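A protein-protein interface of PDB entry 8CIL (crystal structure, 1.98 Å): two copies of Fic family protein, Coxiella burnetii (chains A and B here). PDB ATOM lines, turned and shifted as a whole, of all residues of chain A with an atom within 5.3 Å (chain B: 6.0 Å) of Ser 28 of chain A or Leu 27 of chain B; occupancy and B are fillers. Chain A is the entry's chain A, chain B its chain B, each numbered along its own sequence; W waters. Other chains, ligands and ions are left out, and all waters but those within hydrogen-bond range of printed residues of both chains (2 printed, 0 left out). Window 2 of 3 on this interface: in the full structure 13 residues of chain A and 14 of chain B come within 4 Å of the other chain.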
ATOM      1  N   LEU A  23     -37.691  12.393 -11.105  1.00  0.00           N
ATOM      2  CA  LEU A  23     -37.068  13.427 -11.970  1.00  0.00           C
ATOM      3  C   LEU A  23     -35.887  12.846 -12.752  1.00  0.00           C
ATOM      4  O   LEU A  23     -35.587  13.376 -13.812  1.00  0.00           O
ATOM      5  CB  LEU A  23     -36.669  14.616 -11.099  1.00  0.00           C
ATOM      6  CG  LEU A  23     -37.800  15.610 -10.863  1.00  0.00           C
ATOM      7  CD1 LEU A  23     -38.910  14.990 -10.043  1.00  0.00           C
ATOM      8  CD2 LEU A  23     -37.272  16.865 -10.199  1.00  0.00           C
ATOM      9  N   SER A  24     -35.294  11.770 -12.251  1.00  0.00           N
ATOM     10  CA  SER A  24     -34.109  11.246 -12.952  1.00  0.00           C
ATOM     11  C   SER A  24     -34.317  11.068 -14.460  1.00  0.00           C
ATOM     12  O   SER A  24     -33.460  11.438 -15.267  1.00  0.00           O
ATOM     13  CB  SER A  24     -33.689   9.896 -12.322  1.00  0.00           C
ATOM     14  OG  SER A  24     -32.598   9.383 -13.084  1.00  0.00           O
ATOM     15  N   SER A  25     -35.405  10.420 -14.863  1.00  0.00           N
ATOM     16  CA  SER A  25     -35.615  10.166 -16.283  1.00  0.00           C
ATOM     17  C   SER A  25     -35.907  11.450 -17.043  1.00  0.00           C
ATOM     18  O   SER A  25     -35.491  11.572 -18.210  1.00  0.00           O
ATOM     19  CB  SER A  25     -36.743   9.141 -16.462  1.00  0.00           C
ATOM     20  OG  SER A  25     -37.926   9.738 -15.937  1.00  0.00           O
ATOM     21  N   HIS A  26     -36.499  12.443 -16.396  1.00  0.00           N
ATOM     22  CA  HIS A  26     -36.712  13.738 -17.086  1.00  0.00           C
ATOM     23  C   HIS A  26     -35.363  14.434 -17.316  1.00  0.00           C
ATOM     24  O   HIS A  26     -35.144  14.926 -18.417  1.00  0.00           O
ATOM     25  CB  HIS A  26     -37.694  14.594 -16.291  1.00  0.00           C
ATOM     26  CG  HIS A  26     -39.102  14.089 -16.295  1.00  0.00           C
ATOM     27  ND1 HIS A  26     -39.711  13.536 -15.201  1.00  0.00           N
ATOM     28  CD2 HIS A  26     -39.996  14.037 -17.318  1.00  0.00           C
ATOM     29  CE1 HIS A  26     -40.945  13.174 -15.527  1.00  0.00           C
ATOM     30  NE2 HIS A  26     -41.145  13.478 -16.833  1.00  0.00           N
ATOM     31  N   LEU A  27     -34.488  14.425 -16.320  1.00  0.00           N
ATOM     32  CA  LEU A  27     -33.156  15.073 -16.433  1.00  0.00           C
ATOM     33  C   LEU A  27     -32.303  14.384 -17.501  1.00  0.00           C
ATOM     34  O   LEU A  27     -31.696  15.084 -18.305  1.00  0.00           O
ATOM     35  CB  LEU A  27     -32.490  15.034 -15.061  1.00  0.00           C
ATOM     36  CG  LEU A  27     -33.064  15.989 -14.019  1.00  0.00           C
ATOM     37  CD1 LEU A  27     -32.438  15.735 -12.662  1.00  0.00           C
ATOM     38  CD2 LEU A  27     -32.842  17.431 -14.438  1.00  0.00           C
ATOM     39  N   SER A  28     -32.283  13.061 -17.499  1.00  0.00           N
ATOM     40  CA  SER A  28     -31.494  12.299 -18.489  1.00  0.00           C
ATOM     41  C   SER A  28     -31.983  12.638 -19.897  1.00  0.00           C
ATOM     42  O   SER A  28     -31.151  12.923 -20.759  1.00  0.00           O
ATOM     43  CB  SER A  28     -31.567  10.825 -18.199  1.00  0.00           C
ATOM     44  OG  SER A  28     -30.693  10.480 -17.145  1.00  0.00           O
ATOM     45  N   SER A  29     -33.293  12.636 -20.095  1.00  0.00           N
ATOM     46  CA  SER A  29     -33.882  12.956 -21.413  1.00  0.00           C
ATOM     47  C   SER A  29     -33.547  14.398 -21.805  1.00  0.00           C
ATOM     48  O   SER A  29     -33.248  14.631 -22.964  1.00  0.00           O
ATOM     49  CB  SER A  29     -35.361  12.730 -21.400  1.00  0.00           C
ATOM     50  OG  SER A  29     -35.970  13.431 -20.334  1.00  0.00           O
ATOM     51  N   ALA A  30     -33.614  15.314 -20.847  1.00  0.00           N
ATOM     52  CA  ALA A  30     -33.269  16.699 -21.162  1.00  0.00           C
ATOM     53  C   ALA A  30     -31.793  16.851 -21.550  1.00  0.00           C
ATOM     54  O   ALA A  30     -31.457  17.595 -22.486  1.00  0.00           O
ATOM     55  CB  ALA A  30     -33.580  17.627 -19.971  1.00  0.00           C
ATOM     56  N   ARG A  31     -30.895  16.189 -20.812  1.00  0.00           N
ATOM     57  CA  ARG A  31     -29.472  16.271 -21.134  1.00  0.00           C
ATOM     58  C   ARG A  31     -29.182  15.719 -22.528  1.00  0.00           C
ATOM     59  O   ARG A  31     -28.305  16.226 -23.235  1.00  0.00           O
ATOM     60  CB  ARG A  31     -28.638  15.492 -20.092  1.00  0.00           C
ATOM     61  CG  ARG A  31     -28.608  16.173 -18.752  1.00  0.00           C
ATOM     62  CD  ARG A  31     -28.237  17.593 -18.796  1.00  0.00           C
ATOM     63  NE  ARG A  31     -27.991  18.153 -17.457  1.00  0.00           N
ATOM     64  CZ  ARG A  31     -27.440  19.357 -17.238  1.00  0.00           C
ATOM     65  NH1 ARG A  31     -27.087  20.114 -18.277  1.00  0.00           N
ATOM     66  NH2 ARG A  31     -27.186  19.798 -15.998  1.00  0.00           N
ATOM     67  N   LEU A  32     -29.864  14.649 -22.917  1.00  0.00           N
ATOM     68  CA  LEU A  32     -29.634  14.073 -24.242  1.00  0.00           C
ATOM     69  C   LEU A  32     -29.955  15.091 -25.352  1.00  0.00           C
ATOM     70  O   LEU A  32     -29.171  15.247 -26.294  1.00  0.00           O
ATOM     71  CB  LEU A  32     -30.492  12.833 -24.423  1.00  0.00           C
ATOM     72  CG  LEU A  32     -30.392  12.080 -25.756  1.00  0.00           C
ATOM     73  CD1 LEU A  32     -28.943  11.498 -26.000  1.00  0.00           C
ATOM     74  CD2 LEU A  32     -31.433  10.889 -25.852  1.00  0.00           C
ATOM     75  N   LEU B  23     -27.389   6.845  -9.164  1.00  0.00           N
ATOM     76  CA  LEU B  23     -27.130   6.698 -10.585  1.00  0.00           C
ATOM     77  C   LEU B  23     -27.637   7.878 -11.434  1.00  0.00           C
ATOM     78  O   LEU B  23     -27.144   8.082 -12.549  1.00  0.00           O
ATOM     79  CB  LEU B  23     -27.764   5.420 -11.084  1.00  0.00           C
ATOM     80  CG  LEU B  23     -26.745   4.306 -10.871  1.00  0.00           C
ATOM     81  CD1 LEU B  23     -27.456   3.089 -11.090  1.00  0.00           C
ATOM     82  CD2 LEU B  23     -25.598   4.452 -11.885  1.00  0.00           C
ATOM     83  N   SER B  24     -28.621   8.626 -10.934  1.00  0.00           N
ATOM     84  CA  SER B  24     -29.232   9.709 -11.686  1.00  0.00           C
ATOM     85  C   SER B  24     -28.197  10.686 -12.269  1.00  0.00           C
ATOM     86  O   SER B  24     -28.240  11.000 -13.462  1.00  0.00           O
ATOM     87  CB  SER B  24     -30.186  10.468 -10.767  1.00  0.00           C
ATOM     88  OG  SER B  24     -30.727  11.607 -11.460  1.00  0.00           O
ATOM     89  N   SER B  25     -27.286  11.212 -11.446  1.00  0.00           N
ATOM     90  CA  SER B  25     -26.347  12.170 -12.024  1.00  0.00           C
ATOM     91  C   SER B  25     -25.338  11.495 -12.983  1.00  0.00           C
ATOM     92  O   SER B  25     -24.885  12.159 -13.906  1.00  0.00           O
ATOM     93  CB  SER B  25     -25.610  12.965 -10.930  1.00  0.00           C
ATOM     94  OG  SER B  25     -24.760  12.043 -10.242  1.00  0.00           O
ATOM     95  N   HIS B  26     -24.948  10.191 -12.783  1.00  0.00           N
ATOM     96  CA  HIS B  26     -24.075   9.507 -13.757  1.00  0.00           C
ATOM     97  C   HIS B  26     -24.764   9.375 -15.095  1.00  0.00           C
ATOM     98  O   HIS B  26     -24.156   9.612 -16.139  1.00  0.00           O
ATOM     99  CB  HIS B  26     -23.707   8.096 -13.262  1.00  0.00           C
ATOM    100  CG  HIS B  26     -22.824   8.122 -12.067  1.00  0.00           C
ATOM    101  ND1 HIS B  26     -23.314   8.103 -10.772  1.00  0.00           N
ATOM    102  CD2 HIS B  26     -21.497   8.310 -11.962  1.00  0.00           C
ATOM    103  CE1 HIS B  26     -22.318   8.225  -9.922  1.00  0.00           C
ATOM    104  NE2 HIS B  26     -21.200   8.336 -10.619  1.00  0.00           N
ATOM    105  N   LEU B  27     -26.052   8.999 -15.079  1.00  0.00           N
ATOM    106  CA  LEU B  27     -26.791   8.801 -16.323  1.00  0.00           C
ATOM    107  C   LEU B  27     -26.989  10.123 -17.044  1.00  0.00           C
ATOM    108  O   LEU B  27     -26.897  10.177 -18.277  1.00  0.00           O
ATOM    109  CB  LEU B  27     -28.175   8.169 -16.050  1.00  0.00           C
ATOM    110  CG  LEU B  27     -28.216   6.694 -15.695  1.00  0.00           C
ATOM    111  CD1 LEU B  27     -29.652   6.367 -15.129  1.00  0.00           C
ATOM    112  CD2 LEU B  27     -27.787   5.820 -17.019  1.00  0.00           C
ATOM    113  N   SER B  28     -27.409  11.169 -16.322  1.00  0.00           N
ATOM    114  CA  SER B  28     -27.653  12.415 -17.054  1.00  0.00           C
ATOM    115  C   SER B  28     -26.328  12.978 -17.629  1.00  0.00           C
ATOM    116  O   SER B  28     -26.314  13.552 -18.724  1.00  0.00           O
ATOM    117  CB  SER B  28     -28.472  13.426 -16.226  1.00  0.00           C
ATOM    118  OG  SER B  28     -27.735  13.849 -15.135  1.00  0.00           O
ATOM    119  N   SER B  29     -25.211  12.856 -16.908  1.00  0.00           N
ATOM    120  CA  SER B  29     -23.959  13.320 -17.493  1.00  0.00           C
ATOM    121  C   SER B  29     -23.526  12.432 -18.674  1.00  0.00           C
ATOM    122  O   SER B  29     -22.905  12.928 -19.619  1.00  0.00           O
ATOM    123  CB  SER B  29     -22.866  13.362 -16.438  1.00  0.00           C
ATOM    124  OG  SER B  29     -22.665  12.032 -16.056  1.00  0.00           O
ATOM    125  N   ALA B  30     -23.844  11.143 -18.650  1.00  0.00           N
ATOM    126  CA  ALA B  30     -23.572  10.283 -19.815  1.00  0.00           C
ATOM    127  C   ALA B  30     -24.448  10.682 -21.011  1.00  0.00           C
ATOM    128  O   ALA B  30     -23.995  10.666 -22.155  1.00  0.00           O
ATOM    129  CB  ALA B  30     -23.830   8.808 -19.459  1.00  0.00           C
ATOM    130  N   ARG B  31     -25.739  10.960 -20.767  1.00  0.00           N
ATOM    131  CA  ARG B  31     -26.633  11.404 -21.835  1.00  0.00           C
ATOM    132  C   ARG B  31     -26.164  12.714 -22.452  1.00  0.00           C
ATOM    133  O   ARG B  31     -26.327  12.921 -23.643  1.00  0.00           O
ATOM    134  CB  ARG B  31     -28.067  11.608 -21.313  1.00  0.00           C
ATOM    135  CG  ARG B  31     -28.791  10.279 -20.986  1.00  0.00           C
ATOM    136  CD  ARG B  31     -28.685   9.259 -22.065  1.00  0.00           C
ATOM    137  NE  ARG B  31     -29.616   8.151 -21.820  1.00  0.00           N
ATOM    138  CZ  ARG B  31     -29.945   7.239 -22.740  1.00  0.00           C
ATOM    139  NH1 ARG B  31     -29.368   7.328 -23.955  1.00  0.00           N
ATOM    140  NH2 ARG B  31     -30.842   6.246 -22.448  1.00  0.00           N
ATOM    141  N   LEU B  32     -25.635  13.625 -21.650  1.00  0.00           N
ATOM    142  CA  LEU B  32     -25.168  14.883 -22.193  1.00  0.00           C
ATOM    143  C   LEU B  32     -24.042  14.660 -23.215  1.00  0.00           C
ATOM    144  O   LEU B  32     -24.102  15.191 -24.320  1.00  0.00           O
ATOM    145  CB  LEU B  32     -24.702  15.812 -21.063  1.00  0.00           C
ATOM    146  CG  LEU B  32     -24.106  17.144 -21.500  1.00  0.00           C
ATOM    147  CD1 LEU B  32     -25.250  18.007 -22.220  1.00  0.00           C
ATOM    148  CD2 LEU B  32     -23.648  18.031 -20.304  1.00  0.00           C
ATOM    149  N   ASP B 191     -34.063   2.513 -18.903  1.00  0.00           N
ATOM    150  CA  ASP B 191     -33.177   3.455 -19.618  1.00  0.00           C
ATOM    151  C   ASP B 191     -32.212   2.630 -20.461  1.00  0.00           C
ATOM    152  O   ASP B 191     -31.658   1.658 -19.953  1.00  0.00           O
ATOM    153  CB  ASP B 191     -32.431   4.371 -18.657  1.00  0.00           C
ATOM    154  CG  ASP B 191     -31.330   5.174 -19.324  1.00  0.00           C
ATOM    155  OD1 ASP B 191     -30.267   4.596 -19.586  1.00  0.00           O
ATOM    156  OD2 ASP B 191     -31.560   6.361 -19.593  1.00  0.00           O
ATOM    157  N   LEU B 193     -29.185   3.032 -21.394  1.00  0.00           N
ATOM    158  CA  LEU B 193     -27.794   2.845 -20.944  1.00  0.00           C
ATOM    159  C   LEU B 193     -27.729   1.828 -19.810  1.00  0.00           C
ATOM    160  O   LEU B 193     -26.767   1.061 -19.703  1.00  0.00           O
ATOM    161  CB  LEU B 193     -27.168   4.174 -20.474  1.00  0.00           C
ATOM    162  CG  LEU B 193     -27.120   5.287 -21.559  1.00  0.00           C
ATOM    163  CD1 LEU B 193     -26.451   6.598 -21.062  1.00  0.00           C
ATOM    164  CD2 LEU B 193     -26.355   4.741 -22.763  1.00  0.00           C
ATOM    165  N   LEU B 194     -28.747   1.817 -18.958  1.00  0.00           N
ATOM    166  CA  LEU B 194     -28.788   0.835 -17.844  1.00  0.00           C
ATOM    167  C   LEU B 194     -29.002  -0.567 -18.423  1.00  0.00           C
ATOM    168  O   LEU B 194     -28.349  -1.500 -17.953  1.00  0.00           O
ATOM    169  CB  LEU B 194     -29.900   1.226 -16.867  1.00  0.00           C
ATOM    170  CG  LEU B 194     -29.609   2.434 -15.979  1.00  0.00           C
ATOM    171  CD1 LEU B 194     -30.684   2.590 -14.918  1.00  0.00           C
ATOM    172  CD2 LEU B 194     -28.241   2.308 -15.332  1.00  0.00           C
ATOM    173  N   ILE B 271     -20.978   3.000 -16.808  1.00  0.00           N
ATOM    174  CA  ILE B 271     -21.342   4.322 -17.393  1.00  0.00           C
ATOM    175  C   ILE B 271     -20.055   5.125 -17.619  1.00  0.00           C
ATOM    176  O   ILE B 271     -19.969   5.829 -18.609  1.00  0.00           O
ATOM    177  CB  ILE B 271     -22.361   5.069 -16.513  1.00  0.00           C
ATOM    178  CG1 ILE B 271     -23.725   4.376 -16.507  1.00  0.00           C
ATOM    179  CG2 ILE B 271     -22.474   6.525 -16.934  1.00  0.00           C
ATOM    180  CD1 ILE B 271     -24.641   4.850 -15.414  1.00  0.00           C
ATOM    181  N   LYS B 275     -18.700   6.655 -21.075  1.00  0.00           N
ATOM    182  CA  LYS B 275     -18.238   8.059 -21.208  1.00  0.00           C
ATOM    183  C   LYS B 275     -16.832   8.094 -21.821  1.00  0.00           C
ATOM    184  O   LYS B 275     -16.589   8.947 -22.676  1.00  0.00           O
ATOM    185  CB  LYS B 275     -18.249   8.751 -19.846  1.00  0.00           C
ATOM    186  CG  LYS B 275     -19.611   9.069 -19.248  1.00  0.00           C
ATOM    187  CD  LYS B 275     -19.458   9.934 -18.019  1.00  0.00           C
ATOM    188  CE  LYS B 275     -20.663   9.938 -17.106  1.00  0.00           C
ATOM    189  NZ  LYS B 275     -20.373  10.668 -15.851  1.00  0.00           N
HETATM  190  O   HOH W   1     -31.585   7.132 -11.702  1.00  0.00           O
HETATM  191  O   HOH W   2     -30.695  11.232 -14.825  1.00  0.00           O
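The side-chain hydroxyl (OG) of Ser 24 of chain A sits at hydrogen-bond distance from the side-chain hydroxyl (OG) of Ser 24 of chain B, at 3.3 Å.
OG of Ser 28 of chain A sits at hydrogen-bond distance from N of Ser 28 of chain B (3.5 Å).
O of Ser 24 of chain B is in hydrogen-bond range of OG of Ser 28 of chain B (3.3 Å).
NH2 of Arg 31 of chain B lies within salt-bridge range of OD2 of Asp 191 of chain B.
The side-chain hydroxyl of Ser 28 of chain A is in hydrogen-bond range of the backbone carbonyl oxygen of Ser 24 of chain A (3.5 Å).
Among the printed residues, merely in contact across the chains: Ser 28 of chain A with Leu 27 of chain B (3.6 Å), Ser 28 of chain A with Arg 31 of chain B (3.4 Å), Arg 31 of chain A with Ser 28 of chain B (3.3 Å), Arg 31 of chain A with Arg 31 of chain B (3.9 Å), Arg 31 of chain A with Leu 32 of chain B (3.6 Å) and Leu 32 of chain A with Arg 31 of chain B (3.6 Å).
Of chain B, only Leu 27 (3.6 Å), Ser 28 (3.5 Å) and Arg 31 (3.4 Å) come within 4 Å of Ser 28 of chain A.
Leu 27 of chain B touches just one residue of chain A: Ser 28.
Of the printed residues of chain A, Ser 24 of chain B touches Ser 24 (3.3 Å).
Of the printed residues of chain A, Arg 31 of chain B touches Ser 28, Arg 31 and Leu 32.
Of the printed residues of chain A, Leu 32 of chain B touches Arg 31 (3.6 Å).
Of the printed residues of chain B, Leu 32 of chain A touches Arg 31 (3.6 Å).
Ala 30 of chain A touches none of the printed residues of chain B.
Leu 27 of chain A touches none of the printed residues of chain B.
The nearest residue of chain B that does not touch Ser 28 of chain A is Ser 24 of chain B (4.5 Å).
The nearest printed residue of chain B that does not touch Ser 24 of chain A is Leu 27 of chain B (4.7 Å).
Of the 10 printed residues of chain A, 4 touch a printed residue of chain B.
Printed residues of chain A that touch a printed residue of chain B: Ser 24, Ser 28, Arg 31 and Leu 32.
Among the printed residues, 8 pairs touch across the chains.
Among the printed residues, no Asp or Glu carboxylate lies within 4 Å of a Lys or Arg side-chain nitrogen of the other chain.
Ser 24 of chain B touches its own counterpart, Ser 24 of chain A.
Ser 28 of chain A touches Leu 27 of chain B, but with the chains exchanged Leu 27 of chain A does not touch Ser 28 of chain B (4.1 Å).
Ser 28 of chain A touches its own counterpart, Ser 28 of chain B.
Arg 31 of chain A touches Leu 32 of chain B, and with the chains exchanged Leu 32 of chain A touches Arg 31 of chain B.
Of the 8 pairs that touch across the chains among the printed residues, 7 have their exchanged pair printed and touching as well.
Water W2 lies within hydrogen-bond range of the side-chain hydroxyl of Ser 28 of chain A, the backbone carbonyl oxygen of Ser 24 of chain A and the backbone carbonyl oxygen of Ser 24 of chain B.
Water W1 lies within hydrogen-bond range of the side-chain hydroxyl (OG) of Ser 24 of chain A (2.8 Å) and the backbone NH (N) of Ser 24 of chain B (3.4 Å).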
